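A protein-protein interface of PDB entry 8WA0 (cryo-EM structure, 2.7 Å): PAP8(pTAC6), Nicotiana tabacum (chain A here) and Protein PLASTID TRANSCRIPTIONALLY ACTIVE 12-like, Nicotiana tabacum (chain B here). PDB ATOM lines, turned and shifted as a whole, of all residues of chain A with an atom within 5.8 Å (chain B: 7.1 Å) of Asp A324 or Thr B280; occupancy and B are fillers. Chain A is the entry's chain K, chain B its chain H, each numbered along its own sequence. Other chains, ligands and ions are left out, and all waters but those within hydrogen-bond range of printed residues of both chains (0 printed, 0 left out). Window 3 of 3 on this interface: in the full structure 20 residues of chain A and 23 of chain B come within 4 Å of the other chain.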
ATOM      1  N   LEU A 322      -7.722  21.487 -22.964  1.00  0.00           N
ATOM      2  CA  LEU A 322      -8.116  20.250 -22.382  1.00  0.00           C
ATOM      3  C   LEU A 322      -9.503  19.868 -22.848  1.00  0.00           C
ATOM      4  O   LEU A 322     -10.333  20.731 -23.031  1.00  0.00           O
ATOM      5  CB  LEU A 322      -7.926  20.322 -20.885  1.00  0.00           C
ATOM      6  CG  LEU A 322      -6.538  20.658 -20.369  1.00  0.00           C
ATOM      7  CD1 LEU A 322      -6.531  20.584 -18.857  1.00  0.00           C
ATOM      8  CD2 LEU A 322      -5.502  19.718 -20.943  1.00  0.00           C
ATOM      9  N   ARG A 323      -9.781  18.586 -23.028  1.00  0.00           N
ATOM     10  CA  ARG A 323     -11.048  18.114 -23.587  1.00  0.00           C
ATOM     11  C   ARG A 323     -12.229  18.163 -22.684  1.00  0.00           C
ATOM     12  O   ARG A 323     -13.329  17.854 -23.100  1.00  0.00           O
ATOM     13  CB  ARG A 323     -10.889  16.679 -24.068  1.00  0.00           C
ATOM     14  CG  ARG A 323      -9.618  16.411 -24.840  1.00  0.00           C
ATOM     15  CD  ARG A 323      -9.888  15.510 -26.027  1.00  0.00           C
ATOM     16  NE  ARG A 323      -9.914  14.096 -25.684  1.00  0.00           N
ATOM     17  CZ  ARG A 323      -9.054  13.206 -26.157  1.00  0.00           C
ATOM     18  NH1 ARG A 323      -8.102  13.581 -26.993  1.00  0.00           N
ATOM     19  NH2 ARG A 323      -9.154  11.938 -25.802  1.00  0.00           N
ATOM     20  N   ASP A 324     -12.033  18.525 -21.447  1.00  0.00           N
ATOM     21  CA  ASP A 324     -13.092  18.576 -20.504  1.00  0.00           C
ATOM     22  C   ASP A 324     -13.489  19.978 -20.141  1.00  0.00           C
ATOM     23  O   ASP A 324     -14.256  20.151 -19.215  1.00  0.00           O
ATOM     24  CB  ASP A 324     -12.647  17.861 -19.283  1.00  0.00           C
ATOM     25  CG  ASP A 324     -12.534  16.372 -19.480  1.00  0.00           C
ATOM     26  OD1 ASP A 324     -12.982  15.863 -20.528  1.00  0.00           O
ATOM     27  OD2 ASP A 324     -12.004  15.701 -18.571  1.00  0.00           O
ATOM     28  N   PHE A 325     -13.010  20.990 -20.832  1.00  0.00           N
ATOM     29  CA  PHE A 325     -13.275  22.385 -20.524  1.00  0.00           C
ATOM     30  C   PHE A 325     -14.691  22.831 -20.591  1.00  0.00           C
ATOM     31  O   PHE A 325     -15.113  23.632 -19.783  1.00  0.00           O
ATOM     32  CB  PHE A 325     -12.444  23.240 -21.422  1.00  0.00           C
ATOM     33  CG  PHE A 325     -12.358  24.681 -21.052  1.00  0.00           C
ATOM     34  CD1 PHE A 325     -11.562  25.095 -20.012  1.00  0.00           C
ATOM     35  CD2 PHE A 325     -12.991  25.630 -21.819  1.00  0.00           C
ATOM     36  CE1 PHE A 325     -11.449  26.431 -19.707  1.00  0.00           C
ATOM     37  CE2 PHE A 325     -12.889  26.962 -21.521  1.00  0.00           C
ATOM     38  CZ  PHE A 325     -12.116  27.366 -20.464  1.00  0.00           C
ATOM     39  N   SER A 326     -15.449  22.337 -21.523  1.00  0.00           N
ATOM     40  CA  SER A 326     -16.822  22.700 -21.651  1.00  0.00           C
ATOM     41  C   SER A 326     -17.620  22.299 -20.455  1.00  0.00           C
ATOM     42  O   SER A 326     -18.558  22.976 -20.089  1.00  0.00           O
ATOM     43  CB  SER A 326     -17.378  22.110 -22.906  1.00  0.00           C
ATOM     44  OG  SER A 326     -18.710  22.532 -23.113  1.00  0.00           O
ATOM     45  N   VAL A 327     -17.282  21.186 -19.852  1.00  0.00           N
ATOM     46  CA  VAL A 327     -17.981  20.690 -18.706  1.00  0.00           C
ATOM     47  C   VAL A 327     -17.351  21.033 -17.349  1.00  0.00           C
ATOM     48  O   VAL A 327     -17.571  20.320 -16.393  1.00  0.00           O
ATOM     49  CB  VAL A 327     -18.238  19.201 -18.844  1.00  0.00           C
ATOM     50  CG1 VAL A 327     -19.163  18.932 -20.007  1.00  0.00           C
ATOM     51  CG2 VAL A 327     -16.943  18.430 -19.012  1.00  0.00           C
ATOM     52  N   SER A 328     -16.575  22.103 -17.249  1.00  0.00           N
ATOM     53  CA  SER A 328     -15.931  22.511 -16.005  1.00  0.00           C
ATOM     54  C   SER A 328     -16.388  23.843 -15.408  1.00  0.00           C
ATOM     55  O   SER A 328     -17.087  24.574 -16.069  1.00  0.00           O
ATOM     56  CB  SER A 328     -14.455  22.541 -16.258  1.00  0.00           C
ATOM     57  OG  SER A 328     -14.022  21.368 -16.878  1.00  0.00           O
ATOM     58  N   PHE B 218     -17.671  27.688 -16.990  1.00  0.00           N
ATOM     59  CA  PHE B 218     -16.756  28.338 -17.916  1.00  0.00           C
ATOM     60  C   PHE B 218     -17.380  28.791 -19.211  1.00  0.00           C
ATOM     61  O   PHE B 218     -17.082  29.884 -19.663  1.00  0.00           O
ATOM     62  CB  PHE B 218     -15.629  27.408 -18.292  1.00  0.00           C
ATOM     63  CG  PHE B 218     -14.375  27.560 -17.500  1.00  0.00           C
ATOM     64  CD1 PHE B 218     -13.705  28.753 -17.450  1.00  0.00           C
ATOM     65  CD2 PHE B 218     -13.823  26.464 -16.876  1.00  0.00           C
ATOM     66  CE1 PHE B 218     -12.532  28.868 -16.740  1.00  0.00           C
ATOM     67  CE2 PHE B 218     -12.655  26.567 -16.165  1.00  0.00           C
ATOM     68  CZ  PHE B 218     -12.006  27.769 -16.102  1.00  0.00           C
ATOM     69  N   ARG B 254      -9.527   6.286 -14.011  1.00  0.00           N
ATOM     70  CA  ARG B 254      -8.871   7.528 -13.652  1.00  0.00           C
ATOM     71  C   ARG B 254      -7.942   7.434 -12.490  1.00  0.00           C
ATOM     72  O   ARG B 254      -8.242   6.742 -11.540  1.00  0.00           O
ATOM     73  CB  ARG B 254      -9.954   8.537 -13.310  1.00  0.00           C
ATOM     74  CG  ARG B 254      -9.575   9.993 -13.524  1.00  0.00           C
ATOM     75  CD  ARG B 254     -10.799  10.876 -13.387  1.00  0.00           C
ATOM     76  NE  ARG B 254     -10.481  12.295 -13.306  1.00  0.00           N
ATOM     77  CZ  ARG B 254     -10.279  12.948 -12.169  1.00  0.00           C
ATOM     78  NH1 ARG B 254     -10.349  12.310 -11.009  1.00  0.00           N
ATOM     79  NH2 ARG B 254     -10.001  14.240 -12.187  1.00  0.00           N
ATOM     80  N   THR B 260      -8.332  15.534  -6.106  1.00  0.00           N
ATOM     81  CA  THR B 260      -9.680  15.075  -6.192  1.00  0.00           C
ATOM     82  C   THR B 260     -10.325  14.886  -4.833  1.00  0.00           C
ATOM     83  O   THR B 260     -11.457  15.286  -4.641  1.00  0.00           O
ATOM     84  CB  THR B 260      -9.782  13.812  -7.040  1.00  0.00           C
ATOM     85  OG1 THR B 260      -9.177  14.032  -8.314  1.00  0.00           O
ATOM     86  CG2 THR B 260     -11.216  13.406  -7.247  1.00  0.00           C
ATOM     87  N   LEU B 263     -11.106  18.452  -3.381  1.00  0.00           N
ATOM     88  CA  LEU B 263     -12.150  19.158  -4.066  1.00  0.00           C
ATOM     89  C   LEU B 263     -13.493  18.605  -3.685  1.00  0.00           C
ATOM     90  O   LEU B 263     -14.426  19.352  -3.475  1.00  0.00           O
ATOM     91  CB  LEU B 263     -11.942  19.148  -5.559  1.00  0.00           C
ATOM     92  CG  LEU B 263     -11.052  20.239  -6.128  1.00  0.00           C
ATOM     93  CD1 LEU B 263     -10.918  20.052  -7.624  1.00  0.00           C
ATOM     94  CD2 LEU B 263     -11.664  21.590  -5.815  1.00  0.00           C
ATOM     95  N   LEU B 274     -18.952  22.860  -8.067  1.00  0.00           N
ATOM     96  CA  LEU B 274     -18.350  22.330  -9.251  1.00  0.00           C
ATOM     97  C   LEU B 274     -19.431  21.833 -10.177  1.00  0.00           C
ATOM     98  O   LEU B 274     -20.488  21.442  -9.705  1.00  0.00           O
ATOM     99  CB  LEU B 274     -17.486  21.164  -8.855  1.00  0.00           C
ATOM    100  CG  LEU B 274     -16.428  21.186  -7.761  1.00  0.00           C
ATOM    101  CD1 LEU B 274     -16.009  19.761  -7.474  1.00  0.00           C
ATOM    102  CD2 LEU B 274     -15.231  22.029  -8.148  1.00  0.00           C
ATOM    103  N   TYR B 275     -19.219  21.846 -11.475  1.00  0.00           N
ATOM    104  CA  TYR B 275     -20.179  21.341 -12.421  1.00  0.00           C
ATOM    105  C   TYR B 275     -20.073  19.921 -12.085  1.00  0.00           C
ATOM    106  O   TYR B 275     -18.974  19.375 -12.114  1.00  0.00           O
ATOM    107  CB  TYR B 275     -19.575  21.557 -13.796  1.00  0.00           C
ATOM    108  CG  TYR B 275     -20.440  21.515 -15.014  1.00  0.00           C
ATOM    109  CD1 TYR B 275     -21.019  20.341 -15.446  1.00  0.00           C
ATOM    110  CD2 TYR B 275     -20.606  22.643 -15.786  1.00  0.00           C
ATOM    111  CE1 TYR B 275     -21.785  20.311 -16.588  1.00  0.00           C
ATOM    112  CE2 TYR B 275     -21.365  22.620 -16.928  1.00  0.00           C
ATOM    113  CZ  TYR B 275     -21.952  21.452 -17.321  1.00  0.00           C
ATOM    114  OH  TYR B 275     -22.713  21.437 -18.459  1.00  0.00           O
ATOM    115  N   HIS B 278     -18.389  14.703  -9.750  1.00  0.00           N
ATOM    116  CA  HIS B 278     -17.019  14.263  -9.658  1.00  0.00           C
ATOM    117  C   HIS B 278     -16.179  15.273 -10.330  1.00  0.00           C
ATOM    118  O   HIS B 278     -16.542  15.747 -11.381  1.00  0.00           O
ATOM    119  CB  HIS B 278     -16.822  12.923 -10.315  1.00  0.00           C
ATOM    120  CG  HIS B 278     -15.556  12.230  -9.929  1.00  0.00           C
ATOM    121  ND1 HIS B 278     -15.489  11.332  -8.889  1.00  0.00           N
ATOM    122  CD2 HIS B 278     -14.310  12.288 -10.456  1.00  0.00           C
ATOM    123  CE1 HIS B 278     -14.255  10.876  -8.782  1.00  0.00           C
ATOM    124  NE2 HIS B 278     -13.520  11.442  -9.720  1.00  0.00           N
ATOM    125  N   PRO B 279     -15.051  15.626  -9.744  1.00  0.00           N
ATOM    126  CA  PRO B 279     -14.155  16.614 -10.309  1.00  0.00           C
ATOM    127  C   PRO B 279     -13.569  16.244 -11.643  1.00  0.00           C
ATOM    128  O   PRO B 279     -13.308  15.073 -11.875  1.00  0.00           O
ATOM    129  CB  PRO B 279     -13.083  16.678  -9.264  1.00  0.00           C
ATOM    130  CG  PRO B 279     -13.771  16.410  -7.992  1.00  0.00           C
ATOM    131  CD  PRO B 279     -14.716  15.323  -8.346  1.00  0.00           C
ATOM    132  N   THR B 280     -13.355  17.189 -12.516  1.00  0.00           N
ATOM    133  CA  THR B 280     -12.805  16.958 -13.816  1.00  0.00           C
ATOM    134  C   THR B 280     -11.344  17.277 -13.821  1.00  0.00           C
ATOM    135  O   THR B 280     -10.834  17.807 -12.858  1.00  0.00           O
ATOM    136  CB  THR B 280     -13.558  17.790 -14.843  1.00  0.00           C
ATOM    137  OG1 THR B 280     -13.404  17.213 -16.137  1.00  0.00           O
ATOM    138  CG2 THR B 280     -13.050  19.159 -14.860  1.00  0.00           C
ATOM    139  N   LEU B 281     -10.631  16.913 -14.856  1.00  0.00           N
ATOM    140  CA  LEU B 281      -9.221  17.175 -14.941  1.00  0.00           C
ATOM    141  C   LEU B 281      -8.862  18.644 -14.989  1.00  0.00           C
ATOM    142  O   LEU B 281      -7.868  19.036 -14.396  1.00  0.00           O
ATOM    143  CB  LEU B 281      -8.518  16.302 -15.971  1.00  0.00           C
ATOM    144  CG  LEU B 281      -8.370  14.822 -15.663  1.00  0.00           C
ATOM    145  CD1 LEU B 281      -8.036  14.050 -16.920  1.00  0.00           C
ATOM    146  CD2 LEU B 281      -7.295  14.623 -14.611  1.00  0.00           C
ATOM    147  N   THR B 282      -9.618  19.478 -15.663  1.00  0.00           N
ATOM    148  CA  THR B 282      -9.389  20.910 -15.612  1.00  0.00           C
ATOM    149  C   THR B 282      -9.626  21.485 -14.227  1.00  0.00           C
ATOM    150  O   THR B 282      -8.908  22.377 -13.817  1.00  0.00           O
ATOM    151  CB  THR B 282     -10.077  21.712 -16.746  1.00  0.00           C
ATOM    152  N   GLU B 283     -10.613  21.015 -13.504  1.00  0.00           N
ATOM    153  CA  GLU B 283     -10.853  21.471 -12.174  1.00  0.00           C
ATOM    154  C   GLU B 283      -9.732  21.127 -11.250  1.00  0.00           C
ATOM    155  O   GLU B 283      -9.339  21.939 -10.436  1.00  0.00           O
ATOM    156  CB  GLU B 283     -12.170  20.974 -11.688  1.00  0.00           C
ATOM    157  CG  GLU B 283     -13.361  21.692 -12.275  1.00  0.00           C
ATOM    158  CD  GLU B 283     -14.651  20.953 -12.038  1.00  0.00           C
ATOM    159  OE1 GLU B 283     -14.633  19.934 -11.327  1.00  0.00           O
ATOM    160  OE2 GLU B 283     -15.686  21.377 -12.567  1.00  0.00           O
ATOM    161  N   THR B 284      -9.162  19.957 -11.380  1.00  0.00           N
ATOM    162  CA  THR B 284      -8.009  19.569 -10.594  1.00  0.00           C
ATOM    163  C   THR B 284      -6.796  20.419 -10.866  1.00  0.00           C
ATOM    164  O   THR B 284      -6.067  20.740  -9.942  1.00  0.00           O
ATOM    165  CB  THR B 284      -7.765  18.054 -10.611  1.00  0.00           C
ATOM    166  OG1 THR B 284      -7.625  17.590 -11.951  1.00  0.00           O
ATOM    167  CG2 THR B 284      -8.898  17.330  -9.954  1.00  0.00           C
ATOM    168  N   ALA B 285      -6.565  20.818 -12.094  1.00  0.00           N
ATOM    169  CA  ALA B 285      -5.494  21.724 -12.431  1.00  0.00           C
ATOM    170  C   ALA B 285      -5.611  23.097 -11.840  1.00  0.00           C
ATOM    171  O   ALA B 285      -4.625  23.636 -11.359  1.00  0.00           O
ATOM    172  CB  ALA B 285      -5.389  21.815 -13.894  1.00  0.00           C
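Among the printed residues, merely in contact across the chains: Ser A328 with Thr B280 (3.1 Å), Val A327 with Tyr B275 (3.4 Å), Ser A328 with Glu B283 (3.6 Å), Phe A325 with Phe B218 (3.7 Å) and Ser A328 with Thr B282 (3.96 Å).
The side-chain carboxylate of Asp A324 lies within hydrogen-bond range of the side-chain hydroxyl of Thr B280 (3.2 Å). O of Ser A328 sits at hydrogen-bond distance from N of Phe B218 (3.3 Å).
The backbone carbonyl oxygen (O) of Asp A324 lies within hydrogen-bond range of the side-chain hydroxyl (OG) of Ser A328 (2.6 Å). The side-chain carboxylate (OE1) of Glu B283 sits at hydrogen-bond distance from the backbone NH (N) of Thr B280. O of Thr B280 sits at hydrogen-bond distance from OG1 of Thr B284, at 3.3 Å.
Asp A324 touches just one residue of chain B: Thr B280. Thr B280 touches two residues of chain A. Of the printed residues of chain B, Ser A328 touches Phe B218 (3.3 Å), Thr B280 (3.1 Å), Thr B282 (3.96 Å) and Glu B283 (3.6 Å). Of the printed residues of chain A, Thr B282 touches Ser A328. Thr B284 touches none of the printed residues of chain A. Leu A322 touches none of the printed residues of chain B. The nearest residue of chain B that does not touch Asp A324 is Leu B281 (4.1 Å).
Of the 7 printed residues of chain A, 4 touch a printed residue of chain B. Hydrophobic or aromatic side chains of chain B that line the printed part of chain A: Phe B218 and Tyr B275. Among the printed residues, 7 pairs touch across the chains. Among the printed residues, no Asp or Glu carboxylate lies within 4 Å of a Lys or Arg side-chain nitrogen of the other chain.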
